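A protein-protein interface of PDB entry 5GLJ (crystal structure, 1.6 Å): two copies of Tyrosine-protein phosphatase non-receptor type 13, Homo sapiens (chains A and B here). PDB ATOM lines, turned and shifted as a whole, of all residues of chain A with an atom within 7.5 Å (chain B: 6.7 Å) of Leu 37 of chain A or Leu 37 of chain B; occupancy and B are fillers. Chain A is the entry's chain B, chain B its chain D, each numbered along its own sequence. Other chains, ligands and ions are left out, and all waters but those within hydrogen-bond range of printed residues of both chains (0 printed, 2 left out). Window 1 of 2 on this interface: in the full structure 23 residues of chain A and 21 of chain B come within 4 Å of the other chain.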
ATOM      1  N   ILE A   9     -14.692   0.578 -16.458  1.00  0.00           N
ATOM      2  CA  ILE A   9     -14.886   1.059 -15.094  1.00  0.00           C
ATOM      3  C   ILE A   9     -15.716   0.042 -14.331  1.00  0.00           C
ATOM      4  O   ILE A   9     -16.763  -0.400 -14.825  1.00  0.00           O
ATOM      5  CB  ILE A   9     -15.595   2.429 -15.077  1.00  0.00           C
ATOM      6  CG1 ILE A   9     -14.803   3.443 -15.910  1.00  0.00           C
ATOM      7  CG2 ILE A   9     -15.862   2.910 -13.640  1.00  0.00           C
ATOM      8  CD1 ILE A   9     -13.442   3.762 -15.389  1.00  0.00           C
ATOM      9  N   MET A  32       0.967  15.274  -7.529  1.00  0.00           N
ATOM     10  CA  MET A  32      -0.297  15.107  -8.234  1.00  0.00           C
ATOM     11  C   MET A  32      -0.940  16.444  -8.519  1.00  0.00           C
ATOM     12  O   MET A  32      -1.113  17.246  -7.605  1.00  0.00           O
ATOM     13  CB  MET A  32      -1.260  14.263  -7.395  1.00  0.00           C
ATOM     14  CG  MET A  32      -1.920  13.117  -8.121  1.00  0.00           C
ATOM     15  SD  MET A  32      -0.723  11.930  -8.730  1.00  0.00           S
ATOM     16  CE  MET A  32       0.393  11.875  -7.314  1.00  0.00           C
ATOM     17  N   GLY A  33      -1.311  16.675  -9.771  1.00  0.00           N
ATOM     18  CA  GLY A  33      -2.173  17.798 -10.089  1.00  0.00           C
ATOM     19  C   GLY A  33      -3.567  17.513  -9.567  1.00  0.00           C
ATOM     20  O   GLY A  33      -3.897  16.363  -9.284  1.00  0.00           O
ATOM     21  N   ARG A  34      -4.388  18.556  -9.469  1.00  0.00           N
ATOM     22  CA  ARG A  34      -5.705  18.478  -8.851  1.00  0.00           C
ATOM     23  C   ARG A  34      -6.597  17.390  -9.447  1.00  0.00           C
ATOM     24  O   ARG A  34      -7.418  16.808  -8.744  1.00  0.00           O
ATOM     25  CB  ARG A  34      -6.400  19.841  -8.965  1.00  0.00           C
ATOM     26  CG  ARG A  34      -7.799  19.890  -8.385  1.00  0.00           C
ATOM     27  CD  ARG A  34      -8.397  21.294  -8.508  1.00  0.00           C
ATOM     28  NE  ARG A  34      -8.470  21.729  -9.900  1.00  0.00           N
ATOM     29  CZ  ARG A  34      -9.552  21.614 -10.661  1.00  0.00           C
ATOM     30  NH1 ARG A  34     -10.662  21.086 -10.161  1.00  0.00           N
ATOM     31  NH2 ARG A  34      -9.529  22.032 -11.918  1.00  0.00           N
ATOM     32  N   LEU A  35      -6.423  17.118 -10.737  1.00  0.00           N
ATOM     33  CA  LEU A  35      -7.267  16.152 -11.446  1.00  0.00           C
ATOM     34  C   LEU A  35      -6.503  14.886 -11.819  1.00  0.00           C
ATOM     35  O   LEU A  35      -7.035  14.019 -12.504  1.00  0.00           O
ATOM     36  CB  LEU A  35      -7.863  16.789 -12.706  1.00  0.00           C
ATOM     37  CG  LEU A  35      -8.855  17.925 -12.430  1.00  0.00           C
ATOM     38  CD1 LEU A  35      -9.421  18.482 -13.728  1.00  0.00           C
ATOM     39  CD2 LEU A  35      -9.969  17.449 -11.502  1.00  0.00           C
ATOM     40  N   ASP A  36      -5.254  14.777 -11.380  1.00  0.00           N
ATOM     41  CA  ASP A  36      -4.458  13.598 -11.720  1.00  0.00           C
ATOM     42  C   ASP A  36      -4.928  12.371 -10.946  1.00  0.00           C
ATOM     43  O   ASP A  36      -5.264  12.467  -9.764  1.00  0.00           O
ATOM     44  CB  ASP A  36      -2.971  13.829 -11.437  1.00  0.00           C
ATOM     45  CG  ASP A  36      -2.321  14.792 -12.415  1.00  0.00           C
ATOM     46  OD1 ASP A  36      -2.884  15.049 -13.496  1.00  0.00           O
ATOM     47  OD2 ASP A  36      -1.223  15.285 -12.095  1.00  0.00           O
ATOM     48  N   LEU A  37      -4.953  11.228 -11.629  1.00  0.00           N
ATOM     49  CA  LEU A  37      -5.224   9.941 -11.004  1.00  0.00           C
ATOM     50  C   LEU A  37      -4.014   9.029 -11.178  1.00  0.00           C
ATOM     51  O   LEU A  37      -3.864   8.355 -12.200  1.00  0.00           O
ATOM     52  CB  LEU A  37      -6.475   9.303 -11.613  1.00  0.00           C
ATOM     53  CG  LEU A  37      -7.764   9.937 -11.081  1.00  0.00           C
ATOM     54  CD1 LEU A  37      -8.921   9.700 -12.047  1.00  0.00           C
ATOM     55  CD2 LEU A  37      -8.078   9.388  -9.683  1.00  0.00           C
ATOM     56  N   GLY A  38      -3.133   9.019 -10.189  1.00  0.00           N
ATOM     57  CA  GLY A  38      -1.871   8.327 -10.371  1.00  0.00           C
ATOM     58  C   GLY A  38      -1.670   7.112  -9.495  1.00  0.00           C
ATOM     59  O   GLY A  38      -0.536   6.665  -9.307  1.00  0.00           O
ATOM     60  N   ILE A  39      -2.758   6.581  -8.942  1.00  0.00           N
ATOM     61  CA  ILE A  39      -2.657   5.449  -8.030  1.00  0.00           C
ATOM     62  C   ILE A  39      -3.060   4.169  -8.744  1.00  0.00           C
ATOM     63  O   ILE A  39      -4.149   4.085  -9.300  1.00  0.00           O
ATOM     64  CB  ILE A  39      -3.541   5.638  -6.773  1.00  0.00           C
ATOM     65  CG1 ILE A  39      -3.228   6.979  -6.094  1.00  0.00           C
ATOM     66  CG2 ILE A  39      -3.367   4.458  -5.800  1.00  0.00           C
ATOM     67  CD1 ILE A  39      -1.806   7.089  -5.604  1.00  0.00           C
ATOM     68  N   PHE A  40      -2.165   3.183  -8.734  1.00  0.00           N
ATOM     69  CA  PHE A  40      -2.409   1.904  -9.404  1.00  0.00           C
ATOM     70  C   PHE A  40      -2.094   0.715  -8.499  1.00  0.00           C
ATOM     71  O   PHE A  40      -1.314   0.832  -7.564  1.00  0.00           O
ATOM     72  CB  PHE A  40      -1.568   1.785 -10.684  1.00  0.00           C
ATOM     73  CG  PHE A  40      -1.873   2.844 -11.725  1.00  0.00           C
ATOM     74  CD1 PHE A  40      -1.353   4.129 -11.606  1.00  0.00           C
ATOM     75  CD2 PHE A  40      -2.666   2.547 -12.833  1.00  0.00           C
ATOM     76  CE1 PHE A  40      -1.622   5.102 -12.556  1.00  0.00           C
ATOM     77  CE2 PHE A  40      -2.938   3.518 -13.791  1.00  0.00           C
ATOM     78  CZ  PHE A  40      -2.415   4.794 -13.652  1.00  0.00           C
ATOM     79  N   ARG A  61      -6.463   0.799 -12.008  1.00  0.00           N
ATOM     80  CA  ARG A  61      -6.281   2.173 -11.558  1.00  0.00           C
ATOM     81  C   ARG A  61      -7.318   2.492 -10.502  1.00  0.00           C
ATOM     82  O   ARG A  61      -8.512   2.261 -10.719  1.00  0.00           O
ATOM     83  CB  ARG A  61      -6.382   3.124 -12.750  1.00  0.00           C
ATOM     84  CG  ARG A  61      -6.081   4.583 -12.459  1.00  0.00           C
ATOM     85  CD  ARG A  61      -6.452   5.426 -13.678  1.00  0.00           C
ATOM     86  NE  ARG A  61      -5.674   6.656 -13.777  1.00  0.00           N
ATOM     87  CZ  ARG A  61      -5.759   7.497 -14.799  1.00  0.00           C
ATOM     88  NH1 ARG A  61      -6.601   7.248 -15.796  1.00  0.00           N
ATOM     89  NH2 ARG A  61      -5.014   8.600 -14.820  1.00  0.00           N
ATOM     90  N   LEU A  62      -6.876   2.997  -9.351  1.00  0.00           N
ATOM     91  CA  LEU A  62      -7.796   3.253  -8.248  1.00  0.00           C
ATOM     92  C   LEU A  62      -8.387   4.657  -8.329  1.00  0.00           C
ATOM     93  O   LEU A  62      -7.676   5.667  -8.228  1.00  0.00           O
ATOM     94  CB  LEU A  62      -7.099   3.036  -6.907  1.00  0.00           C
ATOM     95  CG  LEU A  62      -7.950   3.087  -5.636  1.00  0.00           C
ATOM     96  CD1 LEU A  62      -9.132   2.095  -5.677  1.00  0.00           C
ATOM     97  CD2 LEU A  62      -7.080   2.834  -4.412  1.00  0.00           C
ATOM     98  N   ILE A  63      -9.702   4.716  -8.490  1.00  0.00           N
ATOM     99  CA  ILE A  63     -10.366   5.997  -8.721  1.00  0.00           C
ATOM    100  C   ILE A  63     -11.041   6.553  -7.462  1.00  0.00           C
ATOM    101  O   ILE A  63     -10.973   7.752  -7.210  1.00  0.00           O
ATOM    102  CB  ILE A  63     -11.371   5.880  -9.876  1.00  0.00           C
ATOM    103  CG1 ILE A  63     -10.595   5.552 -11.157  1.00  0.00           C
ATOM    104  CG2 ILE A  63     -12.164   7.182 -10.040  1.00  0.00           C
ATOM    105  CD1 ILE A  63     -11.435   5.383 -12.376  1.00  0.00           C
ATOM    106  N   SER A  64     -11.668   5.700  -6.663  1.00  0.00           N
ATOM    107  CA  SER A  64     -12.226   6.191  -5.399  1.00  0.00           C
ATOM    108  C   SER A  64     -12.308   5.115  -4.332  1.00  0.00           C
ATOM    109  O   SER A  64     -12.342   3.918  -4.630  1.00  0.00           O
ATOM    110  CB  SER A  64     -13.615   6.806  -5.604  1.00  0.00           C
ATOM    111  OG  SER A  64     -14.567   5.859  -6.069  1.00  0.00           O
ATOM    112  N   SER A  69     -12.818  10.603  -4.017  1.00  0.00           N
ATOM    113  CA  SER A  69     -11.988  10.558  -5.214  1.00  0.00           C
ATOM    114  C   SER A  69     -10.494  10.610  -4.885  1.00  0.00           C
ATOM    115  O   SER A  69     -10.072  11.312  -3.965  1.00  0.00           O
ATOM    116  CB  SER A  69     -12.344  11.712  -6.144  1.00  0.00           C
ATOM    117  OG  SER A  69     -11.462  11.728  -7.245  1.00  0.00           O
ATOM    118  N   LEU A  70      -9.698   9.878  -5.658  1.00  0.00           N
ATOM    119  CA  LEU A  70      -8.250   9.927  -5.525  1.00  0.00           C
ATOM    120  C   LEU A  70      -7.641  10.925  -6.507  1.00  0.00           C
ATOM    121  O   LEU A  70      -6.420  10.944  -6.702  1.00  0.00           O
ATOM    122  CB  LEU A  70      -7.648   8.544  -5.742  1.00  0.00           C
ATOM    123  CG  LEU A  70      -7.992   7.550  -4.624  1.00  0.00           C
ATOM    124  CD1 LEU A  70      -7.034   6.398  -4.631  1.00  0.00           C
ATOM    125  CD2 LEU A  70      -7.997   8.232  -3.247  1.00  0.00           C
ATOM    126  N   GLU A  71      -8.485  11.752  -7.117  1.00  0.00           N
ATOM    127  CA  GLU A  71      -8.006  12.852  -7.950  1.00  0.00           C
ATOM    128  C   GLU A  71      -7.155  13.793  -7.109  1.00  0.00           C
ATOM    129  O   GLU A  71      -7.591  14.271  -6.065  1.00  0.00           O
ATOM    130  CB  GLU A  71      -9.173  13.614  -8.588  1.00  0.00           C
ATOM    131  CG  GLU A  71      -9.818  12.887  -9.753  1.00  0.00           C
ATOM    132  CD  GLU A  71     -11.219  13.393 -10.038  1.00  0.00           C
ATOM    133  OE1 GLU A  71     -11.565  13.597 -11.220  1.00  0.00           O
ATOM    134  OE2 GLU A  71     -11.984  13.586  -9.069  1.00  0.00           O
ATOM    135  N   GLY A  72      -5.929  14.029  -7.562  1.00  0.00           N
ATOM    136  CA  GLY A  72      -5.017  14.912  -6.861  1.00  0.00           C
ATOM    137  C   GLY A  72      -4.415  14.316  -5.607  1.00  0.00           C
ATOM    138  O   GLY A  72      -3.792  15.025  -4.823  1.00  0.00           O
ATOM    139  N   VAL A  73      -4.596  13.016  -5.407  1.00  0.00           N
ATOM    140  CA  VAL A  73      -4.145  12.389  -4.172  1.00  0.00           C
ATOM    141  C   VAL A  73      -2.811  11.667  -4.376  1.00  0.00           C
ATOM    142  O   VAL A  73      -2.661  10.869  -5.293  1.00  0.00           O
ATOM    143  CB  VAL A  73      -5.214  11.416  -3.620  1.00  0.00           C
ATOM    144  CG1 VAL A  73      -4.714  10.718  -2.366  1.00  0.00           C
ATOM    145  CG2 VAL A  73      -6.528  12.185  -3.339  1.00  0.00           C
ATOM    146  N   SER A  94     -10.579   1.563 -12.671  1.00  0.00           N
ATOM    147  CA  SER A  94     -10.578   1.338 -14.110  1.00  0.00           C
ATOM    148  C   SER A  94      -9.602   0.212 -14.417  1.00  0.00           C
ATOM    149  O   SER A  94      -8.623  -0.008 -13.696  1.00  0.00           O
ATOM    150  CB  SER A  94     -10.231   2.602 -14.911  1.00  0.00           C
ATOM    151  OG  SER A  94      -8.870   2.987 -14.769  1.00  0.00           O
ATOM    152  N   ILE B   9     -16.667  10.841  -6.121  1.00  0.00           N
ATOM    153  CA  ILE B   9     -17.220  10.115  -7.252  1.00  0.00           C
ATOM    154  C   ILE B   9     -18.708   9.920  -7.019  1.00  0.00           C
ATOM    155  O   ILE B   9     -19.144   9.686  -5.886  1.00  0.00           O
ATOM    156  CB  ILE B   9     -16.512   8.762  -7.441  1.00  0.00           C
ATOM    157  CG1 ILE B   9     -15.016   8.986  -7.704  1.00  0.00           C
ATOM    158  CG2 ILE B   9     -17.181   7.926  -8.539  1.00  0.00           C
ATOM    159  CD1 ILE B   9     -14.678   9.781  -8.926  1.00  0.00           C
ATOM    160  N   GLY B  29     -11.500  16.250 -24.668  1.00  0.00           N
ATOM    161  CA  GLY B  29     -11.029  15.000 -25.232  1.00  0.00           C
ATOM    162  C   GLY B  29      -9.646  14.755 -24.676  1.00  0.00           C
ATOM    163  O   GLY B  29      -9.052  15.649 -24.072  1.00  0.00           O
ATOM    164  N   GLU B  30      -9.127  13.548 -24.857  1.00  0.00           N
ATOM    165  CA  GLU B  30      -7.783  13.271 -24.386  1.00  0.00           C
ATOM    166  C   GLU B  30      -6.775  14.102 -25.157  1.00  0.00           C
ATOM    167  O   GLU B  30      -6.939  14.347 -26.358  1.00  0.00           O
ATOM    168  CB  GLU B  30      -7.440  11.779 -24.517  1.00  0.00           C
ATOM    169  CG  GLU B  30      -7.333  11.270 -25.943  1.00  0.00           C
ATOM    170  CD  GLU B  30      -5.975  11.514 -26.602  1.00  0.00           C
ATOM    171  OE1 GLU B  30      -4.997  11.903 -25.926  1.00  0.00           O
ATOM    172  OE2 GLU B  30      -5.901  11.334 -27.830  1.00  0.00           O
ATOM    173  N   GLY B  33      -3.015  11.081 -23.980  1.00  0.00           N
ATOM    174  CA  GLY B  33      -3.017   9.659 -24.268  1.00  0.00           C
ATOM    175  C   GLY B  33      -3.981   8.788 -23.479  1.00  0.00           C
ATOM    176  O   GLY B  33      -4.968   9.268 -22.914  1.00  0.00           O
ATOM    177  N   ARG B  34      -3.648   7.496 -23.431  1.00  0.00           N
ATOM    178  CA  ARG B  34      -4.522   6.409 -22.978  1.00  0.00           C
ATOM    179  C   ARG B  34      -5.184   6.555 -21.605  1.00  0.00           C
ATOM    180  O   ARG B  34      -6.282   6.021 -21.383  1.00  0.00           O
ATOM    181  CB  ARG B  34      -3.712   5.101 -23.000  1.00  0.00           C
ATOM    182  CG  ARG B  34      -4.458   3.863 -22.507  1.00  0.00           C
ATOM    183  CD  ARG B  34      -5.666   3.502 -23.379  1.00  0.00           C
ATOM    184  NE  ARG B  34      -6.001   2.083 -23.221  1.00  0.00           N
ATOM    185  CZ  ARG B  34      -7.100   1.498 -23.691  1.00  0.00           C
ATOM    186  NH1 ARG B  34      -8.010   2.199 -24.347  1.00  0.00           N
ATOM    187  NH2 ARG B  34      -7.292   0.197 -23.493  1.00  0.00           N
ATOM    188  N   LEU B  35      -4.530   7.251 -20.685  1.00  0.00           N
ATOM    189  CA  LEU B  35      -5.049   7.372 -19.326  1.00  0.00           C
ATOM    190  C   LEU B  35      -5.710   8.723 -19.069  1.00  0.00           C
ATOM    191  O   LEU B  35      -6.232   8.957 -17.987  1.00  0.00           O
ATOM    192  CB  LEU B  35      -3.929   7.149 -18.305  1.00  0.00           C
ATOM    193  CG  LEU B  35      -3.364   5.734 -18.373  1.00  0.00           C
ATOM    194  CD1 LEU B  35      -2.157   5.572 -17.438  1.00  0.00           C
ATOM    195  CD2 LEU B  35      -4.461   4.733 -18.056  1.00  0.00           C
ATOM    196  N   ASP B  36      -5.672   9.609 -20.058  1.00  0.00           N
ATOM    197  CA  ASP B  36      -6.167  10.975 -19.889  1.00  0.00           C
ATOM    198  C   ASP B  36      -7.701  11.007 -19.869  1.00  0.00           C
ATOM    199  O   ASP B  36      -8.349  10.489 -20.782  1.00  0.00           O
ATOM    200  CB  ASP B  36      -5.610  11.857 -21.016  1.00  0.00           C
ATOM    201  CG  ASP B  36      -5.781  13.354 -20.763  1.00  0.00           C
ATOM    202  OD1 ASP B  36      -6.187  13.761 -19.657  1.00  0.00           O
ATOM    203  OD2 ASP B  36      -5.472  14.131 -21.691  1.00  0.00           O
ATOM    204  N   LEU B  37      -8.268  11.602 -18.821  1.00  0.00           N
ATOM    205  CA  LEU B  37      -9.707  11.807 -18.721  1.00  0.00           C
ATOM    206  C   LEU B  37      -9.998  13.269 -18.991  1.00  0.00           C
ATOM    207  O   LEU B  37      -9.968  14.090 -18.078  1.00  0.00           O
ATOM    208  CB  LEU B  37     -10.225  11.384 -17.344  1.00  0.00           C
ATOM    209  CG  LEU B  37     -10.428   9.875 -17.182  1.00  0.00           C
ATOM    210  CD1 LEU B  37     -10.227   9.435 -15.719  1.00  0.00           C
ATOM    211  CD2 LEU B  37     -11.805   9.467 -17.697  1.00  0.00           C
ATOM    212  N   GLY B  38     -10.264  13.591 -20.254  1.00  0.00           N
ATOM    213  CA  GLY B  38     -10.382  14.977 -20.655  1.00  0.00           C
ATOM    214  C   GLY B  38     -11.790  15.428 -20.958  1.00  0.00           C
ATOM    215  O   GLY B  38     -11.977  16.510 -21.496  1.00  0.00           O
ATOM    216  N   ILE B  39     -12.777  14.605 -20.612  1.00  0.00           N
ATOM    217  CA  ILE B  39     -14.172  14.905 -20.953  1.00  0.00           C
ATOM    218  C   ILE B  39     -14.914  15.532 -19.787  1.00  0.00           C
ATOM    219  O   ILE B  39     -14.928  14.986 -18.683  1.00  0.00           O
ATOM    220  CB  ILE B  39     -14.940  13.630 -21.379  1.00  0.00           C
ATOM    221  CG1 ILE B  39     -14.188  12.864 -22.468  1.00  0.00           C
ATOM    222  CG2 ILE B  39     -16.363  13.986 -21.828  1.00  0.00           C
ATOM    223  CD1 ILE B  39     -13.981  13.654 -23.718  1.00  0.00           C
ATOM    224  N   PHE B  40     -15.554  16.670 -20.035  1.00  0.00           N
ATOM    225  CA  PHE B  40     -16.322  17.352 -19.001  1.00  0.00           C
ATOM    226  C   PHE B  40     -17.722  17.703 -19.502  1.00  0.00           C
ATOM    227  O   PHE B  40     -17.957  17.808 -20.711  1.00  0.00           O
ATOM    228  CB  PHE B  40     -15.583  18.623 -18.530  1.00  0.00           C
ATOM    229  CG  PHE B  40     -14.261  18.333 -17.878  1.00  0.00           C
ATOM    230  CD1 PHE B  40     -13.127  18.138 -18.652  1.00  0.00           C
ATOM    231  CD2 PHE B  40     -14.154  18.251 -16.498  1.00  0.00           C
ATOM    232  CE1 PHE B  40     -11.914  17.843 -18.062  1.00  0.00           C
ATOM    233  CE2 PHE B  40     -12.943  17.956 -15.899  1.00  0.00           C
ATOM    234  CZ  PHE B  40     -11.820  17.756 -16.683  1.00  0.00           C
ATOM    235  N   ARG B  61     -16.780  16.057 -14.243  1.00  0.00           N
ATOM    236  CA  ARG B  61     -15.910  15.256 -15.079  1.00  0.00           C
ATOM    237  C   ARG B  61     -16.575  13.928 -15.400  1.00  0.00           C
ATOM    238  O   ARG B  61     -16.978  13.226 -14.482  1.00  0.00           O
ATOM    239  CB  ARG B  61     -14.583  15.024 -14.367  1.00  0.00           C
ATOM    240  CG  ARG B  61     -13.499  14.410 -15.243  1.00  0.00           C
ATOM    241  CD  ARG B  61     -12.274  14.063 -14.413  1.00  0.00           C
ATOM    242  NE  ARG B  61     -11.050  14.113 -15.194  1.00  0.00           N
ATOM    243  CZ  ARG B  61      -9.839  13.970 -14.656  1.00  0.00           C
ATOM    244  NH1 ARG B  61      -9.728  13.766 -13.354  1.00  0.00           N
ATOM    245  NH2 ARG B  61      -8.749  14.040 -15.411  1.00  0.00           N
ATOM    246  N   LEU B  62     -16.659  13.571 -16.682  1.00  0.00           N
ATOM    247  CA  LEU B  62     -17.302  12.311 -17.077  1.00  0.00           C
ATOM    248  C   LEU B  62     -16.282  11.192 -17.198  1.00  0.00           C
ATOM    249  O   LEU B  62     -15.439  11.205 -18.086  1.00  0.00           O
ATOM    250  CB  LEU B  62     -18.049  12.473 -18.395  1.00  0.00           C
ATOM    251  CG  LEU B  62     -18.903  11.283 -18.843  1.00  0.00           C
ATOM    252  CD1 LEU B  62     -19.882  10.877 -17.748  1.00  0.00           C
ATOM    253  CD2 LEU B  62     -19.657  11.650 -20.119  1.00  0.00           C
ATOM    254  N   ILE B  63     -16.377  10.220 -16.298  1.00  0.00           N
ATOM    255  CA  ILE B  63     -15.393   9.137 -16.248  1.00  0.00           C
ATOM    256  C   ILE B  63     -15.858   7.897 -17.017  1.00  0.00           C
ATOM    257  O   ILE B  63     -15.061   7.249 -17.707  1.00  0.00           O
ATOM    258  CB  ILE B  63     -15.070   8.803 -14.784  1.00  0.00           C
ATOM    259  CG1 ILE B  63     -14.421  10.040 -14.144  1.00  0.00           C
ATOM    260  CG2 ILE B  63     -14.152   7.588 -14.690  1.00  0.00           C
ATOM    261  CD1 ILE B  63     -14.194   9.937 -12.653  1.00  0.00           C
ATOM    262  N   SER B  64     -17.150   7.577 -16.953  1.00  0.00           N
ATOM    263  CA  SER B  64     -17.641   6.410 -17.689  1.00  0.00           C
ATOM    264  C   SER B  64     -19.078   6.565 -18.160  1.00  0.00           C
ATOM    265  O   SER B  64     -19.853   7.327 -17.586  1.00  0.00           O
ATOM    266  CB  SER B  64     -17.544   5.147 -16.827  1.00  0.00           C
ATOM    267  OG  SER B  64     -18.663   5.042 -15.976  1.00  0.00           O
ATOM    268  N   SER B  69     -15.096   3.202 -20.140  1.00  0.00           N
ATOM    269  CA  SER B  69     -14.259   4.274 -19.632  1.00  0.00           C
ATOM    270  C   SER B  69     -13.990   5.333 -20.695  1.00  0.00           C
ATOM    271  O   SER B  69     -13.811   5.014 -21.876  1.00  0.00           O
ATOM    272  CB  SER B  69     -12.931   3.713 -19.121  1.00  0.00           C
ATOM    273  OG  SER B  69     -12.088   4.797 -18.767  1.00  0.00           O
ATOM    274  N   LEU B  70     -13.934   6.593 -20.278  1.00  0.00           N
ATOM    275  CA  LEU B  70     -13.573   7.657 -21.209  1.00  0.00           C
ATOM    276  C   LEU B  70     -12.071   7.971 -21.132  1.00  0.00           C
ATOM    277  O   LEU B  70     -11.588   8.904 -21.767  1.00  0.00           O
ATOM    278  CB  LEU B  70     -14.420   8.909 -20.958  1.00  0.00           C
ATOM    279  CG  LEU B  70     -15.923   8.750 -21.229  1.00  0.00           C
ATOM    280  CD1 LEU B  70     -16.571  10.110 -21.270  1.00  0.00           C
ATOM    281  CD2 LEU B  70     -16.205   7.986 -22.525  1.00  0.00           C
ATOM    282  N   GLU B  71     -11.319   7.164 -20.391  1.00  0.00           N
ATOM    283  CA  GLU B  71      -9.858   7.307 -20.418  1.00  0.00           C
ATOM    284  C   GLU B  71      -9.289   7.199 -21.833  1.00  0.00           C
ATOM    285  O   GLU B  71      -9.527   6.213 -22.531  1.00  0.00           O
ATOM    286  CB  GLU B  71      -9.200   6.242 -19.539  1.00  0.00           C
ATOM    287  CG  GLU B  71      -9.469   6.422 -18.067  1.00  0.00           C
ATOM    288  CD  GLU B  71      -9.220   5.142 -17.294  1.00  0.00           C
ATOM    289  OE1 GLU B  71      -8.507   5.183 -16.281  1.00  0.00           O
ATOM    290  OE2 GLU B  71      -9.760   4.093 -17.710  1.00  0.00           O
ATOM    291  N   GLY B  72      -8.522   8.206 -22.248  1.00  0.00           N
ATOM    292  CA  GLY B  72      -7.862   8.174 -23.543  1.00  0.00           C
ATOM    293  C   GLY B  72      -8.777   8.388 -24.734  1.00  0.00           C
ATOM    294  O   GLY B  72      -8.371   8.208 -25.884  1.00  0.00           O
ATOM    295  N   VAL B  73     -10.018   8.779 -24.473  1.00  0.00           N
ATOM    296  CA  VAL B  73     -11.002   8.900 -25.540  1.00  0.00           C
ATOM    297  C   VAL B  73     -11.018  10.317 -26.126  1.00  0.00           C
ATOM    298  O   VAL B  73     -10.992  11.303 -25.389  1.00  0.00           O
ATOM    299  CB  VAL B  73     -12.403   8.490 -25.018  1.00  0.00           C
ATOM    300  CG1 VAL B  73     -13.495   8.814 -26.018  1.00  0.00           C
ATOM    301  CG2 VAL B  73     -12.398   6.986 -24.682  1.00  0.00           C
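Among the printed residues, pairs that only touch across the chains: Ser 64 of chain A with Ile 9 of chain B (3.3 Å), Ile 9 of chain A with Ser 64 of chain B (3.4 Å), Ile 9 of chain A with Ser 69 of chain B (3.7 Å), Ile 63 of chain A with Ile 9 of chain B (3.8 Å), Phe 40 of chain A with Leu 35 of chain B (3.9 Å), Leu 35 of chain A with Phe 40 of chain B (3.9 Å), Leu 37 of chain A with Leu 37 of chain B (3.9 Å) and Ile 9 of chain A with Ile 63 of chain B (3.95 Å).
O of Leu 35 of chain A lies within hydrogen-bond range of NH1 of Arg 61 of chain B (2.8 Å). NH1 of Arg 61 of chain A lies within hydrogen-bond range of O of Leu 35 of chain B, at 2.8 Å. The side-chain carboxylate (OE1) of Glu 71 of chain B is in salt-bridge range of the guanidinium group (NH1) of Arg 61 of chain A, at 2.9 Å. The side-chain carboxylate (OE1) of Glu 71 of chain A lies within salt-bridge range of the guanidinium group (NH1) of Arg 61 of chain B (2.8 Å). The side-chain hydroxyl (OG) of Ser 94 of chain A lies within hydrogen-bond range of the side-chain carboxylate (OE1) of Glu 71 of chain B (2.7 Å).
Ile 9 of chain A touches Ser 64 of chain B, and with the chains exchanged Ser 64 of chain A touches Ile 9 of chain B. Ile 9 of chain A touches Ser 69 of chain B, but with the chains exchanged Ser 69 of chain A does not touch Ile 9 of chain B (4.1 Å). Leu 37 of chain B touches its own counterpart, Leu 37 of chain A. Arg 61 of chain A touches Glu 71 of chain B, and with the chains exchanged Glu 71 of chain A touches Arg 61 of chain B. 18 positions are printed for both chains.
Of chain B, only Leu 37 comes within 4 Å of Leu 37 of chain A. Of chain A, only Leu 37 comes within 4 Å of Leu 37 of chain B. Of the printed residues of chain A, Ser 69 of chain B touches Ile 9. Printed residues of chain A within 4 Å of Glu 71 of chain B: Arg 61 (2.9 Å) and Ser 94 (2.7 Å). Of the printed residues of chain B, Ile 63 of chain A touches Ile 9 (3.8 Å). Glu 30 of chain B touches none of the printed residues of chain A. The nearest printed residue of chain A that does not touch Ser 64 of chain B is Ile 63 of chain A (7.6 Å).
The backbone carbonyl oxygen of Ser 94 of chain A lies within hydrogen-bond range of the backbone NH of Arg 61 of chain A (2.9 Å). O of Ile 63 of chain A sits at hydrogen-bond distance from N of Leu 70 of chain A (2.9 Å). The side-chain hydroxyl of Ser 69 of chain A is in hydrogen-bond range of the side-chain carboxylate of Glu 71 of chain A, 2.7 Å away. The guanidinium group (NH2) of Arg 61 of chain B is in hydrogen-bond range of the backbone carbonyl oxygen (O) of Leu 37 of chain B (2.9 Å). O of Ile 63 of chain B is in hydrogen-bond range of N of Leu 70 of chain B. OG of Ser 69 of chain B lies within hydrogen-bond range of OE2 of Glu 71 of chain B (2.7 Å).
Hydrophobic or aromatic side chains of chain B that line the printed part of chain A: Ile 9, Leu 35, Leu 37, Phe 40 and Ile 63. Hydrophobic or aromatic side chains of chain A that line the printed part of chain B: Ile 9, Leu 35, Leu 37, Phe 40 and Ile 63. Among the printed residues, Asp or Glu carboxylates within 4 Å of a Lys or Arg side-chain nitrogen of the other chain: Arg 61 of chain A with Glu 71 of chain B (2.9 Å) and Glu 71 of chain A with Arg 61 of chain B (2.8 Å).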
